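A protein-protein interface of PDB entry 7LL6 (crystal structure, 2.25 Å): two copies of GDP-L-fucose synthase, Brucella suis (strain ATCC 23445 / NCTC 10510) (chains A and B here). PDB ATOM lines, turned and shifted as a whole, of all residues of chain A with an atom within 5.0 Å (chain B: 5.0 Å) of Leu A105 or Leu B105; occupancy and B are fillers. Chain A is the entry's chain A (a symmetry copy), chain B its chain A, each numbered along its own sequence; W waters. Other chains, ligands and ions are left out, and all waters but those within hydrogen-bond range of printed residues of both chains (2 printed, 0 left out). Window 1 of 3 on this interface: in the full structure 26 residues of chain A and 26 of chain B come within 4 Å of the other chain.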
ATOM      1  N   LEU A 101     -34.139  -2.490  26.948  1.00  0.00           N
ATOM      2  CA  LEU A 101     -33.454  -2.393  25.659  1.00  0.00           C
ATOM      3  C   LEU A 101     -32.183  -1.561  25.773  1.00  0.00           C
ATOM      4  O   LEU A 101     -31.112  -2.013  25.361  1.00  0.00           O
ATOM      5  CB  LEU A 101     -34.381  -1.792  24.592  1.00  0.00           C
ATOM      6  CG  LEU A 101     -33.930  -2.006  23.131  1.00  0.00           C
ATOM      7  CD1 LEU A 101     -35.123  -1.868  22.163  1.00  0.00           C
ATOM      8  CD2 LEU A 101     -32.783  -1.041  22.692  1.00  0.00           C
ATOM      9  N   TYR A 102     -32.280  -0.350  26.335  1.00  0.00           N
ATOM     10  CA  TYR A 102     -31.152   0.580  26.312  1.00  0.00           C
ATOM     11  C   TYR A 102     -29.980   0.096  27.148  1.00  0.00           C
ATOM     12  O   TYR A 102     -28.835   0.108  26.680  1.00  0.00           O
ATOM     13  CB  TYR A 102     -31.581   1.966  26.820  1.00  0.00           C
ATOM     14  CG  TYR A 102     -30.398   2.916  26.887  1.00  0.00           C
ATOM     15  CD1 TYR A 102     -29.930   3.563  25.742  1.00  0.00           C
ATOM     16  CD2 TYR A 102     -29.729   3.145  28.080  1.00  0.00           C
ATOM     17  CE1 TYR A 102     -28.839   4.422  25.796  1.00  0.00           C
ATOM     18  CE2 TYR A 102     -28.646   3.997  28.143  1.00  0.00           C
ATOM     19  CZ  TYR A 102     -28.206   4.632  27.005  1.00  0.00           C
ATOM     20  OH  TYR A 102     -27.137   5.491  27.096  1.00  0.00           O
ATOM     21  N   ASP A 103     -30.227  -0.264  28.413  1.00  0.00           N
ATOM     22  CA  ASP A 103     -29.129  -0.691  29.280  1.00  0.00           C
ATOM     23  C   ASP A 103     -28.325  -1.806  28.645  1.00  0.00           C
ATOM     24  O   ASP A 103     -27.098  -1.736  28.559  1.00  0.00           O
ATOM     25  CB  ASP A 103     -29.659  -1.152  30.641  1.00  0.00           C
ATOM     26  CG  ASP A 103     -30.071  -0.002  31.511  1.00  0.00           C
ATOM     27  OD1 ASP A 103     -30.009   1.142  31.012  1.00  0.00           O
ATOM     28  OD2 ASP A 103     -30.444  -0.238  32.680  1.00  0.00           O
ATOM     29  N   ASN A 104     -29.001  -2.849  28.180  1.00  0.00           N
ATOM     30  CA  ASN A 104     -28.261  -3.965  27.628  1.00  0.00           C
ATOM     31  C   ASN A 104     -27.599  -3.589  26.306  1.00  0.00           C
ATOM     32  O   ASN A 104     -26.457  -3.997  26.048  1.00  0.00           O
ATOM     33  CB  ASN A 104     -29.182  -5.180  27.481  1.00  0.00           C
ATOM     34  CG  ASN A 104     -29.545  -5.792  28.817  1.00  0.00           C
ATOM     35  OD1 ASN A 104     -28.670  -6.336  29.502  1.00  0.00           O
ATOM     36  ND2 ASN A 104     -30.826  -5.684  29.218  1.00  0.00           N
ATOM     37  N   LEU A 105     -28.281  -2.805  25.450  1.00  0.00           N
ATOM     38  CA  LEU A 105     -27.685  -2.532  24.142  1.00  0.00           C
ATOM     39  C   LEU A 105     -26.490  -1.593  24.269  1.00  0.00           C
ATOM     40  O   LEU A 105     -25.464  -1.789  23.604  1.00  0.00           O
ATOM     41  CB  LEU A 105     -28.732  -1.969  23.175  1.00  0.00           C
ATOM     42  CG  LEU A 105     -28.213  -1.770  21.747  1.00  0.00           C
ATOM     43  CD1 LEU A 105     -27.570  -3.077  21.243  1.00  0.00           C
ATOM     44  CD2 LEU A 105     -29.333  -1.354  20.819  1.00  0.00           C
ATOM     45  N   ALA A 106     -26.577  -0.613  25.159  1.00  0.00           N
ATOM     46  CA  ALA A 106     -25.469   0.324  25.332  1.00  0.00           C
ATOM     47  C   ALA A 106     -24.259  -0.338  25.981  1.00  0.00           C
ATOM     48  O   ALA A 106     -23.118  -0.004  25.636  1.00  0.00           O
ATOM     49  CB  ALA A 106     -25.931   1.527  26.157  1.00  0.00           C
ATOM     50  N   ILE A 107     -24.481  -1.280  26.902  1.00  0.00           N
ATOM     51  CA  ILE A 107     -23.362  -2.042  27.455  1.00  0.00           C
ATOM     52  C   ILE A 107     -22.621  -2.765  26.339  1.00  0.00           C
ATOM     53  O   ILE A 107     -21.389  -2.687  26.233  1.00  0.00           O
ATOM     54  CB  ILE A 107     -23.853  -3.029  28.529  1.00  0.00           C
ATOM     55  CG1 ILE A 107     -24.322  -2.292  29.781  1.00  0.00           C
ATOM     56  CG2 ILE A 107     -22.753  -4.066  28.865  1.00  0.00           C
ATOM     57  CD1 ILE A 107     -25.058  -3.195  30.746  1.00  0.00           C
ATOM     58  N   GLY A 108     -23.360  -3.477  25.483  1.00  0.00           N
ATOM     59  CA  GLY A 108     -22.712  -4.273  24.447  1.00  0.00           C
ATOM     60  C   GLY A 108     -22.037  -3.420  23.386  1.00  0.00           C
ATOM     61  O   GLY A 108     -20.937  -3.742  22.922  1.00  0.00           O
ATOM     62  N   MET A 109     -22.681  -2.321  22.991  1.00  0.00           N
ATOM     63  CA  MET A 109     -22.101  -1.450  21.978  1.00  0.00           C
ATOM     64  C   MET A 109     -20.857  -0.753  22.503  1.00  0.00           C
ATOM     65  O   MET A 109     -19.857  -0.642  21.788  1.00  0.00           O
ATOM     66  CB  MET A 109     -23.116  -0.405  21.529  1.00  0.00           C
ATOM     67  CG  MET A 109     -24.262  -0.980  20.735  1.00  0.00           C
ATOM     68  SD  MET A 109     -24.315  -0.154  19.145  1.00  0.00           S
ATOM     69  CE  MET A 109     -24.190   1.573  19.655  1.00  0.00           C
ATOM     70  N   ASN A 110     -20.919  -0.230  23.728  1.00  0.00           N
ATOM     71  CA  ASN A 110     -19.754   0.460  24.273  1.00  0.00           C
ATOM     72  C   ASN A 110     -18.591  -0.499  24.484  1.00  0.00           C
ATOM     73  O   ASN A 110     -17.438  -0.138  24.238  1.00  0.00           O
ATOM     74  CB  ASN A 110     -20.100   1.162  25.581  1.00  0.00           C
ATOM     75  CG  ASN A 110     -21.075   2.290  25.385  1.00  0.00           C
ATOM     76  OD1 ASN A 110     -21.227   2.811  24.275  1.00  0.00           O
ATOM     77  ND2 ASN A 110     -21.752   2.672  26.453  1.00  0.00           N
ATOM     78  N   ALA A 160     -32.155  -5.947  22.068  1.00  0.00           N
ATOM     79  CA  ALA A 160     -30.858  -5.500  22.563  1.00  0.00           C
ATOM     80  C   ALA A 160     -29.809  -6.606  22.470  1.00  0.00           C
ATOM     81  O   ALA A 160     -28.684  -6.376  21.995  1.00  0.00           O
ATOM     82  CB  ALA A 160     -30.985  -5.000  24.005  1.00  0.00           C
ATOM     83  N   ALA A 163     -28.878  -7.351  18.726  1.00  0.00           N
ATOM     84  CA  ALA A 163     -28.060  -6.321  18.107  1.00  0.00           C
ATOM     85  C   ALA A 163     -26.621  -6.415  18.585  1.00  0.00           C
ATOM     86  O   ALA A 163     -25.683  -6.315  17.784  1.00  0.00           O
ATOM     87  CB  ALA A 163     -28.650  -4.945  18.424  1.00  0.00           C
ATOM     88  N   GLY A 164     -26.423  -6.632  19.891  1.00  0.00           N
ATOM     89  CA  GLY A 164     -25.073  -6.855  20.379  1.00  0.00           C
ATOM     90  C   GLY A 164     -24.423  -8.054  19.713  1.00  0.00           C
ATOM     91  O   GLY A 164     -23.290  -7.974  19.227  1.00  0.00           O
ATOM     92  N   LEU B 101     -23.429  -1.150  10.799  1.00  0.00           N
ATOM     93  CA  LEU B 101     -24.232  -1.392  11.998  1.00  0.00           C
ATOM     94  C   LEU B 101     -23.961  -0.337  13.063  1.00  0.00           C
ATOM     95  O   LEU B 101     -24.899   0.277  13.576  1.00  0.00           O
ATOM     96  CB  LEU B 101     -23.960  -2.793  12.565  1.00  0.00           C
ATOM     97  CG  LEU B 101     -25.013  -3.316  13.564  1.00  0.00           C
ATOM     98  CD1 LEU B 101     -24.966  -4.855  13.657  1.00  0.00           C
ATOM     99  CD2 LEU B 101     -24.867  -2.699  14.992  1.00  0.00           C
ATOM    100  N   TYR B 102     -22.686  -0.108  13.402  1.00  0.00           N
ATOM    101  CA  TYR B 102     -22.354   0.746  14.541  1.00  0.00           C
ATOM    102  C   TYR B 102     -22.735   2.199  14.311  1.00  0.00           C
ATOM    103  O   TYR B 102     -23.360   2.824  15.176  1.00  0.00           O
ATOM    104  CB  TYR B 102     -20.851   0.674  14.855  1.00  0.00           C
ATOM    105  CG  TYR B 102     -20.478   1.626  15.977  1.00  0.00           C
ATOM    106  CD1 TYR B 102     -20.698   1.284  17.312  1.00  0.00           C
ATOM    107  CD2 TYR B 102     -19.939   2.875  15.708  1.00  0.00           C
ATOM    108  CE1 TYR B 102     -20.371   2.159  18.342  1.00  0.00           C
ATOM    109  CE2 TYR B 102     -19.611   3.749  16.724  1.00  0.00           C
ATOM    110  CZ  TYR B 102     -19.826   3.389  18.034  1.00  0.00           C
ATOM    111  OH  TYR B 102     -19.474   4.268  19.029  1.00  0.00           O
ATOM    112  N   ASP B 103     -22.306   2.781  13.184  1.00  0.00           N
ATOM    113  CA  ASP B 103     -22.599   4.192  12.932  1.00  0.00           C
ATOM    114  C   ASP B 103     -24.082   4.476  13.048  1.00  0.00           C
ATOM    115  O   ASP B 103     -24.499   5.397  13.754  1.00  0.00           O
ATOM    116  CB  ASP B 103     -22.104   4.611  11.545  1.00  0.00           C
ATOM    117  CG  ASP B 103     -20.614   4.779  11.499  1.00  0.00           C
ATOM    118  OD1 ASP B 103     -19.975   4.492  12.534  1.00  0.00           O
ATOM    119  OD2 ASP B 103     -20.090   5.199  10.445  1.00  0.00           O
ATOM    120  N   ASN B 104     -24.904   3.688  12.368  1.00  0.00           N
ATOM    121  CA  ASN B 104     -26.324   3.973  12.401  1.00  0.00           C
ATOM    122  C   ASN B 104     -26.914   3.686  13.776  1.00  0.00           C
ATOM    123  O   ASN B 104     -27.766   4.446  14.257  1.00  0.00           O
ATOM    124  CB  ASN B 104     -27.038   3.187  11.297  1.00  0.00           C
ATOM    125  CG  ASN B 104     -26.734   3.728   9.916  1.00  0.00           C
ATOM    126  OD1 ASN B 104     -27.133   4.855   9.595  1.00  0.00           O
ATOM    127  ND2 ASN B 104     -26.000   2.951   9.097  1.00  0.00           N
ATOM    128  N   LEU B 105     -26.477   2.602  14.445  1.00  0.00           N
ATOM    129  CA  LEU B 105     -27.118   2.273  15.718  1.00  0.00           C
ATOM    130  C   LEU B 105     -26.729   3.270  16.804  1.00  0.00           C
ATOM    131  O   LEU B 105     -27.575   3.687  17.607  1.00  0.00           O
ATOM    132  CB  LEU B 105     -26.784   0.837  16.141  1.00  0.00           C
ATOM    133  CG  LEU B 105     -27.518   0.377  17.404  1.00  0.00           C
ATOM    134  CD1 LEU B 105     -29.032   0.619  17.244  1.00  0.00           C
ATOM    135  CD2 LEU B 105     -27.256  -1.089  17.677  1.00  0.00           C
ATOM    136  N   ALA B 106     -25.479   3.713  16.803  1.00  0.00           N
ATOM    137  CA  ALA B 106     -25.037   4.672  17.815  1.00  0.00           C
ATOM    138  C   ALA B 106     -25.665   6.046  17.611  1.00  0.00           C
ATOM    139  O   ALA B 106     -25.972   6.732  18.595  1.00  0.00           O
ATOM    140  CB  ALA B 106     -23.510   4.770  17.804  1.00  0.00           C
ATOM    141  N   ILE B 107     -25.878   6.456  16.358  1.00  0.00           N
ATOM    142  CA  ILE B 107     -26.601   7.702  16.107  1.00  0.00           C
ATOM    143  C   ILE B 107     -27.989   7.635  16.728  1.00  0.00           C
ATOM    144  O   ILE B 107     -28.412   8.545  17.454  1.00  0.00           O
ATOM    145  CB  ILE B 107     -26.679   7.993  14.598  1.00  0.00           C
ATOM    146  CG1 ILE B 107     -25.308   8.360  14.036  1.00  0.00           C
ATOM    147  CG2 ILE B 107     -27.722   9.100  14.306  1.00  0.00           C
ATOM    148  CD1 ILE B 107     -25.288   8.387  12.524  1.00  0.00           C
ATOM    149  N   GLY B 108     -28.720   6.549  16.460  1.00  0.00           N
ATOM    150  CA  GLY B 108     -30.094   6.456  16.942  1.00  0.00           C
ATOM    151  C   GLY B 108     -30.180   6.324  18.452  1.00  0.00           C
ATOM    152  O   GLY B 108     -31.052   6.925  19.091  1.00  0.00           O
ATOM    153  N   MET B 109     -29.278   5.540  19.046  1.00  0.00           N
ATOM    154  CA  MET B 109     -29.293   5.360  20.491  1.00  0.00           C
ATOM    155  C   MET B 109     -28.915   6.647  21.206  1.00  0.00           C
ATOM    156  O   MET B 109     -29.532   7.004  22.213  1.00  0.00           O
ATOM    157  CB  MET B 109     -28.330   4.252  20.899  1.00  0.00           C
ATOM    158  CG  MET B 109     -28.778   2.876  20.474  1.00  0.00           C
ATOM    159  SD  MET B 109     -28.894   1.845  21.935  1.00  0.00           S
ATOM    160  CE  MET B 109     -27.313   2.204  22.730  1.00  0.00           C
ATOM    161  N   ASN B 110     -27.869   7.326  20.733  1.00  0.00           N
ATOM    162  CA  ASN B 110     -27.460   8.563  21.391  1.00  0.00           C
ATOM    163  C   ASN B 110     -28.524   9.642  21.256  1.00  0.00           C
ATOM    164  O   ASN B 110     -28.764  10.398  22.200  1.00  0.00           O
ATOM    165  CB  ASN B 110     -26.131   9.061  20.835  1.00  0.00           C
ATOM    166  CG  ASN B 110     -24.991   8.136  21.157  1.00  0.00           C
ATOM    167  OD1 ASN B 110     -25.075   7.326  22.086  1.00  0.00           O
ATOM    168  ND2 ASN B 110     -23.921   8.236  20.391  1.00  0.00           N
ATOM    169  N   ALA B 160     -29.293  -2.438  12.712  1.00  0.00           N
ATOM    170  CA  ALA B 160     -29.147  -1.120  13.321  1.00  0.00           C
ATOM    171  C   ALA B 160     -30.440  -0.311  13.227  1.00  0.00           C
ATOM    172  O   ALA B 160     -30.887   0.286  14.220  1.00  0.00           O
ATOM    173  CB  ALA B 160     -27.989  -0.360  12.666  1.00  0.00           C
ATOM    174  N   ALA B 163     -33.216  -1.824  15.560  1.00  0.00           N
ATOM    175  CA  ALA B 163     -32.992  -1.581  16.976  1.00  0.00           C
ATOM    176  C   ALA B 163     -33.334  -0.145  17.337  1.00  0.00           C
ATOM    177  O   ALA B 163     -33.982   0.111  18.359  1.00  0.00           O
ATOM    178  CB  ALA B 163     -31.535  -1.896  17.321  1.00  0.00           C
ATOM    179  N   GLY B 164     -32.927   0.812  16.492  1.00  0.00           N
ATOM    180  CA  GLY B 164     -33.336   2.187  16.724  1.00  0.00           C
ATOM    181  C   GLY B 164     -34.846   2.333  16.732  1.00  0.00           C
ATOM    182  O   GLY B 164     -35.422   2.935  17.645  1.00  0.00           O
HETATM  183  O   HOH W   1     -19.726   3.237  21.340  1.00  0.00           O
HETATM  184  O   HOH W   2     -26.721   6.723  24.912  1.00  0.00           O
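Printed residues of chain B that touch a printed residue of chain A: Leu B105, Ala B106 and Met B109. Among the printed residues, 5 pairs touch across the chains. Among the printed residues, no Asp or Glu carboxylate lies within 4 Å of a Lys or Arg side-chain nitrogen of the other chain.
Leu B105 touches its own counterpart, Leu A105. Leu A105 touches Met B109, and with the chains exchanged Met A109 touches Leu B105. Ala A106 touches Met B109, and with the chains exchanged Met A109 touches Ala B106. Of the 5 pairs that touch across the chains among the printed residues, 5 have their exchanged pair printed and touching as well.
Leu A105 touches Leu B105 (CD2 to CD2, 3.8 Å). Met B109 touches Leu A105. Met B109 touches Ala A106. Met A109 touches Leu B105 (SD to CD2, 3.4 Å). CE of Met A109 touches CA of Ala B106 (3.7 Å).
Water W2 lies within hydrogen-bond range of OH of Tyr A102 and OD1 of Asn B110. Water W1 lies within hydrogen-bond range of OH of Tyr B102 (2.5 Å) and OD1 of Asn A110 (3.3 Å).
Leu A105 touches two residues of chain B. Of chain A, only Leu A105 and Met A109 come within 4 Å of Leu B105. Of the printed residues of chain A, Ala B106 touches Met A109 (3.7 Å). Of the printed residues of chain B, Ala A106 touches Met B109. Of the printed residues of chain B, Met A109 touches Leu B105 (3.4 Å) and Ala B106 (3.7 Å). Printed residues of chain A within 4 Å of Met B109: Leu A105 and Ala A106. The nearest residue of chain A that does not touch Leu B105 is Ala A163 (4.2 Å).
ND2 of Asn B110 sits close to O of Ala B106 (3.1 Å). The backbone carbonyl oxygen (O) of Ala A106 sits close to the side-chain amide nitrogen (ND2) of Asn A110 (3.1 Å).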
